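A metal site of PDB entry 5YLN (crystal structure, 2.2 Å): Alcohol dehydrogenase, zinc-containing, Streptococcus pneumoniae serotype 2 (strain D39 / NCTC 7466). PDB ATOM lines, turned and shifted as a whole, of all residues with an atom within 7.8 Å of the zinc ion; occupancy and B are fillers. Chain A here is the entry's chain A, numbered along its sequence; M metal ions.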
ATOM      1  N   CYS A  92       2.777 -24.766  -5.162  1.00  0.00           N
ATOM      2  CA  CYS A  92       3.365 -23.492  -4.756  1.00  0.00           C
ATOM      3  C   CYS A  92       3.285 -23.330  -3.254  1.00  0.00           C
ATOM      4  O   CYS A  92       2.248 -23.625  -2.644  1.00  0.00           O
ATOM      5  CB  CYS A  92       2.653 -22.321  -5.424  1.00  0.00           C
ATOM      6  SG  CYS A  92       2.508 -22.449  -7.207  1.00  0.00           S
ATOM      7  N   ALA A  93       4.348 -22.780  -2.660  1.00  0.00           N
ATOM      8  CA  ALA A  93       4.461 -22.622  -1.206  1.00  0.00           C
ATOM      9  C   ALA A  93       4.947 -21.214  -0.893  1.00  0.00           C
ATOM     10  O   ALA A  93       6.015 -20.809  -1.353  1.00  0.00           O
ATOM     11  CB  ALA A  93       5.418 -23.662  -0.626  1.00  0.00           C
ATOM     12  N   CYS A  94       4.172 -20.462  -0.105  1.00  0.00           N
ATOM     13  CA  CYS A  94       4.612 -19.121   0.286  1.00  0.00           C
ATOM     14  C   CYS A  94       5.701 -19.164   1.352  1.00  0.00           C
ATOM     15  O   CYS A  94       6.467 -18.202   1.475  1.00  0.00           O
ATOM     16  CB  CYS A  94       3.410 -18.288   0.770  1.00  0.00           C
ATOM     17  SG  CYS A  94       2.850 -18.669   2.511  1.00  0.00           S
ATOM     18  N   GLY A  95       5.791 -20.264   2.124  1.00  0.00           N
ATOM     19  CA  GLY A  95       6.809 -20.474   3.129  1.00  0.00           C
ATOM     20  C   GLY A  95       6.558 -19.803   4.465  1.00  0.00           C
ATOM     21  O   GLY A  95       7.386 -19.948   5.371  1.00  0.00           O
ATOM     22  N   LYS A  96       5.439 -19.093   4.622  1.00  0.00           N
ATOM     23  CA  LYS A  96       5.184 -18.261   5.783  1.00  0.00           C
ATOM     24  C   LYS A  96       3.855 -18.506   6.474  1.00  0.00           C
ATOM     25  O   LYS A  96       3.674 -18.026   7.598  1.00  0.00           O
ATOM     26  CB  LYS A  96       5.243 -16.766   5.410  1.00  0.00           C
ATOM     27  CG  LYS A  96       6.598 -16.210   5.050  1.00  0.00           C
ATOM     28  CD  LYS A  96       6.414 -14.826   4.421  1.00  0.00           C
ATOM     29  CE  LYS A  96       7.688 -14.003   4.404  1.00  0.00           C
ATOM     30  NZ  LYS A  96       7.430 -12.707   3.731  1.00  0.00           N
ATOM     31  N   CYS A  97       2.897 -19.172   5.840  1.00  0.00           N
ATOM     32  CA  CYS A  97       1.555 -19.237   6.402  1.00  0.00           C
ATOM     33  C   CYS A  97       1.439 -20.395   7.404  1.00  0.00           C
ATOM     34  O   CYS A  97       2.384 -21.147   7.634  1.00  0.00           O
ATOM     35  CB  CYS A  97       0.518 -19.384   5.297  1.00  0.00           C
ATOM     36  SG  CYS A  97       0.609 -21.035   4.557  1.00  0.00           S
ATOM     37  N   TYR A  98       0.231 -20.555   7.954  1.00  0.00           N
ATOM     38  CA  TYR A  98      -0.026 -21.577   8.963  1.00  0.00           C
ATOM     39  C   TYR A  98       0.412 -22.969   8.473  1.00  0.00           C
ATOM     40  O   TYR A  98       1.049 -23.721   9.207  1.00  0.00           O
ATOM     41  CB  TYR A  98      -1.506 -21.538   9.345  1.00  0.00           C
ATOM     42  CG  TYR A  98      -1.932 -22.583  10.354  1.00  0.00           C
ATOM     43  CD1 TYR A  98      -2.288 -23.862   9.946  1.00  0.00           C
ATOM     44  CD2 TYR A  98      -2.001 -22.284  11.706  1.00  0.00           C
ATOM     45  CE1 TYR A  98      -2.671 -24.814  10.854  1.00  0.00           C
ATOM     46  CE2 TYR A  98      -2.392 -23.243  12.634  1.00  0.00           C
ATOM     47  CZ  TYR A  98      -2.725 -24.510  12.193  1.00  0.00           C
ATOM     48  OH  TYR A  98      -3.119 -25.471  13.084  1.00  0.00           O
ATOM     49  N   TYR A  99       0.096 -23.303   7.215  1.00  0.00           N
ATOM     50  CA  TYR A  99       0.373 -24.659   6.745  1.00  0.00           C
ATOM     51  C   TYR A  99       1.786 -24.790   6.194  1.00  0.00           C
ATOM     52  O   TYR A  99       2.380 -25.865   6.333  1.00  0.00           O
ATOM     53  CB  TYR A  99      -0.675 -25.093   5.707  1.00  0.00           C
ATOM     54  CG  TYR A  99      -1.980 -25.384   6.390  1.00  0.00           C
ATOM     55  CD1 TYR A  99      -2.037 -26.354   7.399  1.00  0.00           C
ATOM     56  CD2 TYR A  99      -3.142 -24.670   6.082  1.00  0.00           C
ATOM     57  CE1 TYR A  99      -3.221 -26.625   8.057  1.00  0.00           C
ATOM     58  CE2 TYR A  99      -4.327 -24.932   6.741  1.00  0.00           C
ATOM     59  CZ  TYR A  99      -4.354 -25.904   7.738  1.00  0.00           C
ATOM     60  OH  TYR A  99      -5.515 -26.182   8.402  1.00  0.00           O
ATOM     61  N   CYS A 100       2.325 -23.741   5.577  1.00  0.00           N
ATOM     62  CA  CYS A 100       3.720 -23.795   5.136  1.00  0.00           C
ATOM     63  C   CYS A 100       4.677 -23.960   6.314  1.00  0.00           C
ATOM     64  O   CYS A 100       5.711 -24.624   6.205  1.00  0.00           O
ATOM     65  CB  CYS A 100       4.077 -22.530   4.353  1.00  0.00           C
ATOM     66  SG  CYS A 100       3.467 -22.515   2.633  1.00  0.00           S
ATOM     67  N   LYS A 101       4.347 -23.346   7.451  1.00  0.00           N
ATOM     68  CA  LYS A 101       5.179 -23.537   8.631  1.00  0.00           C
ATOM     69  C   LYS A 101       5.198 -24.991   9.082  1.00  0.00           C
ATOM     70  O   LYS A 101       6.167 -25.417   9.725  1.00  0.00           O
ATOM     71  CB  LYS A 101       4.713 -22.604   9.751  1.00  0.00           C
ATOM     72  CG  LYS A 101       5.185 -21.165   9.548  1.00  0.00           C
ATOM     73  CD  LYS A 101       6.715 -21.098   9.511  1.00  0.00           C
ATOM     74  CE  LYS A 101       7.223 -19.679   9.487  1.00  0.00           C
ATOM     75  NZ  LYS A 101       6.562 -18.851  10.523  1.00  0.00           N
ATOM     76  N   ILE A 104       3.285 -28.447   5.109  1.00  0.00           N
ATOM     77  CA  ILE A 104       2.126 -28.943   4.363  1.00  0.00           C
ATOM     78  C   ILE A 104       1.853 -27.990   3.215  1.00  0.00           C
ATOM     79  O   ILE A 104       0.846 -27.281   3.183  1.00  0.00           O
ATOM     80  CB  ILE A 104       0.908 -29.094   5.306  1.00  0.00           C
ATOM     81  CG1 ILE A 104       1.305 -29.906   6.549  1.00  0.00           C
ATOM     82  CG2 ILE A 104      -0.266 -29.766   4.593  1.00  0.00           C
ATOM     83  CD1 ILE A 104       0.216 -29.973   7.568  1.00  0.00           C
ATOM     84  N   TYR A 105       2.767 -27.965   2.228  1.00  0.00           N
ATOM     85  CA  TYR A 105       2.661 -26.985   1.161  1.00  0.00           C
ATOM     86  C   TYR A 105       1.409 -27.198   0.319  1.00  0.00           C
ATOM     87  O   TYR A 105       0.940 -26.264  -0.330  1.00  0.00           O
ATOM     88  CB  TYR A 105       3.913 -27.006   0.277  1.00  0.00           C
ATOM     89  CG  TYR A 105       5.208 -26.802   1.054  1.00  0.00           C
ATOM     90  CD1 TYR A 105       5.269 -25.919   2.127  1.00  0.00           C
ATOM     91  CD2 TYR A 105       6.364 -27.498   0.720  1.00  0.00           C
ATOM     92  CE1 TYR A 105       6.429 -25.730   2.850  1.00  0.00           C
ATOM     93  CE2 TYR A 105       7.541 -27.326   1.440  1.00  0.00           C
ATOM     94  CZ  TYR A 105       7.580 -26.436   2.506  1.00  0.00           C
ATOM     95  OH  TYR A 105       8.746 -26.248   3.236  1.00  0.00           O
ATOM     96  N   HIS A 107      -1.423 -27.196   1.313  1.00  0.00           N
ATOM     97  CA  HIS A 107      -2.522 -26.374   1.801  1.00  0.00           C
ATOM     98  C   HIS A 107      -2.068 -24.974   2.168  1.00  0.00           C
ATOM     99  O   HIS A 107      -2.657 -24.335   3.029  1.00  0.00           O
ATOM    100  CB  HIS A 107      -3.226 -27.079   2.955  1.00  0.00           C
ATOM    101  CG  HIS A 107      -3.910 -28.323   2.514  1.00  0.00           C
ATOM    102  ND1 HIS A 107      -5.138 -28.305   1.884  1.00  0.00           N
ATOM    103  CD2 HIS A 107      -3.508 -29.614   2.508  1.00  0.00           C
ATOM    104  CE1 HIS A 107      -5.481 -29.532   1.546  1.00  0.00           C
ATOM    105  NE2 HIS A 107      -4.509 -30.351   1.921  1.00  0.00           N
ATOM    106  N   CYS A 108      -1.031 -24.475   1.473  1.00  0.00           N
ATOM    107  CA  CYS A 108      -0.616 -23.084   1.648  1.00  0.00           C
ATOM    108  C   CYS A 108      -1.791 -22.138   1.412  1.00  0.00           C
ATOM    109  O   CYS A 108      -2.552 -22.290   0.452  1.00  0.00           O
ATOM    110  CB  CYS A 108       0.539 -22.776   0.686  1.00  0.00           C
ATOM    111  SG  CYS A 108       0.919 -21.013   0.535  1.00  0.00           S
ATOM    112  N   GLU A 109      -1.934 -21.142   2.296  1.00  0.00           N
ATOM    113  CA  GLU A 109      -3.095 -20.242   2.297  1.00  0.00           C
ATOM    114  C   GLU A 109      -2.877 -18.939   1.543  1.00  0.00           C
ATOM    115  O   GLU A 109      -3.746 -18.068   1.569  1.00  0.00           O
ATOM    116  CB  GLU A 109      -3.516 -19.919   3.743  1.00  0.00           C
ATOM    117  CG  GLU A 109      -3.829 -21.148   4.595  1.00  0.00           C
ATOM    118  CD  GLU A 109      -4.301 -20.810   6.020  1.00  0.00           C
ATOM    119  OE1 GLU A 109      -5.296 -21.421   6.490  1.00  0.00           O
ATOM    120  OE2 GLU A 109      -3.678 -19.948   6.686  1.00  0.00           O
ATOM    121  N   ASP A 110      -1.735 -18.757   0.879  1.00  0.00           N
ATOM    122  CA  ASP A 110      -1.406 -17.509   0.199  1.00  0.00           C
ATOM    123  C   ASP A 110      -0.912 -17.857  -1.205  1.00  0.00           C
ATOM    124  O   ASP A 110       0.292 -18.064  -1.393  1.00  0.00           O
ATOM    125  CB  ASP A 110      -0.376 -16.728   1.000  1.00  0.00           C
ATOM    126  CG  ASP A 110       0.153 -15.521   0.264  1.00  0.00           C
ATOM    127  OD1 ASP A 110      -0.536 -15.024  -0.644  1.00  0.00           O
ATOM    128  OD2 ASP A 110       1.285 -15.087   0.582  1.00  0.00           O
ATOM    129  N   GLU A 111      -1.822 -17.904  -2.165  1.00  0.00           N
ATOM    130  CA  GLU A 111      -1.572 -18.349  -3.546  1.00  0.00           C
ATOM    131  C   GLU A 111      -0.680 -19.591  -3.565  1.00  0.00           C
ATOM    132  O   GLU A 111       0.399 -19.615  -4.154  1.00  0.00           O
ATOM    133  CB  GLU A 111      -0.965 -17.222  -4.418  1.00  0.00           C
ATOM    134  CG  GLU A 111      -1.187 -17.491  -5.954  1.00  0.00           C
ATOM    135  CD  GLU A 111      -0.635 -16.410  -6.912  1.00  0.00           C
ATOM    136  OE1 GLU A 111       0.132 -15.531  -6.488  1.00  0.00           O
ATOM    137  OE2 GLU A 111      -0.995 -16.450  -8.122  1.00  0.00           O
ATOM    138  N   GLY A 112      -1.162 -20.629  -2.891  1.00  0.00           N
ATOM    139  CA  GLY A 112      -0.365 -21.824  -2.680  1.00  0.00           C
ATOM    140  C   GLY A 112      -1.195 -23.081  -2.849  1.00  0.00           C
ATOM    141  O   GLY A 112      -2.385 -23.027  -3.114  1.00  0.00           O
ATOM    142  N   GLY A 113      -0.513 -24.214  -2.696  1.00  0.00           N
ATOM    143  CA  GLY A 113      -1.123 -25.494  -2.938  1.00  0.00           C
ATOM    144  C   GLY A 113      -0.950 -25.920  -4.384  1.00  0.00           C
ATOM    145  O   GLY A 113      -0.082 -25.428  -5.105  1.00  0.00           O
ATOM    146  N   HIS A 132       5.926 -17.437  -5.702  1.00  0.00           N
ATOM    147  CA  HIS A 132       6.813 -17.850  -4.605  1.00  0.00           C
ATOM    148  C   HIS A 132       7.991 -18.663  -5.108  1.00  0.00           C
ATOM    149  O   HIS A 132       8.236 -19.798  -4.668  1.00  0.00           O
ATOM    150  CB  HIS A 132       6.034 -18.641  -3.560  1.00  0.00           C
ATOM    151  CG  HIS A 132       4.861 -17.891  -2.998  1.00  0.00           C
ATOM    152  ND1 HIS A 132       4.991 -16.670  -2.383  1.00  0.00           N
ATOM    153  CD2 HIS A 132       3.544 -18.189  -2.992  1.00  0.00           C
ATOM    154  CE1 HIS A 132       3.801 -16.240  -2.001  1.00  0.00           C
ATOM    155  NE2 HIS A 132       2.904 -17.147  -2.365  1.00  0.00           N
HETATM  156 ZN    ZN M   1       1.990 -20.840   2.655  1.00  0.00          ZN
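The backbone NH (N) of Tyr 99 sits close to the side-chain sulfur (SG) of Cys 97 (3.5 Å). The backbone NH (N) of Lys 96 lies close to the side-chain sulfur (SG) of Cys 94 (3.4 Å). The backbone NH of Asp 110 sits close to the side-chain sulfur of Cys 108 (3.5 Å). The side-chain sulfur of Cys 97 sits close to the backbone NH of Glu 109. SG of Cys 100 sits close to N of Gly 95.
Residues that only touch the zinc ion: Gly 95 and Glu 109. Six residues have an atom within 4 Å of the zinc ion: Cys 94, Gly 95, Cys 97, Cys 100, Cys 108 and Glu 109.
The zinc ion is bound by SG of Cys 100. The zinc ion is bound by SG of Cys 94 (2.3 Å). SG of Cys 97 binds the zinc ion (2.4 Å). The zinc ion is bound by SG of Cys 108 (2.4 Å). The zinc ion has four donor atoms within binding distance.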
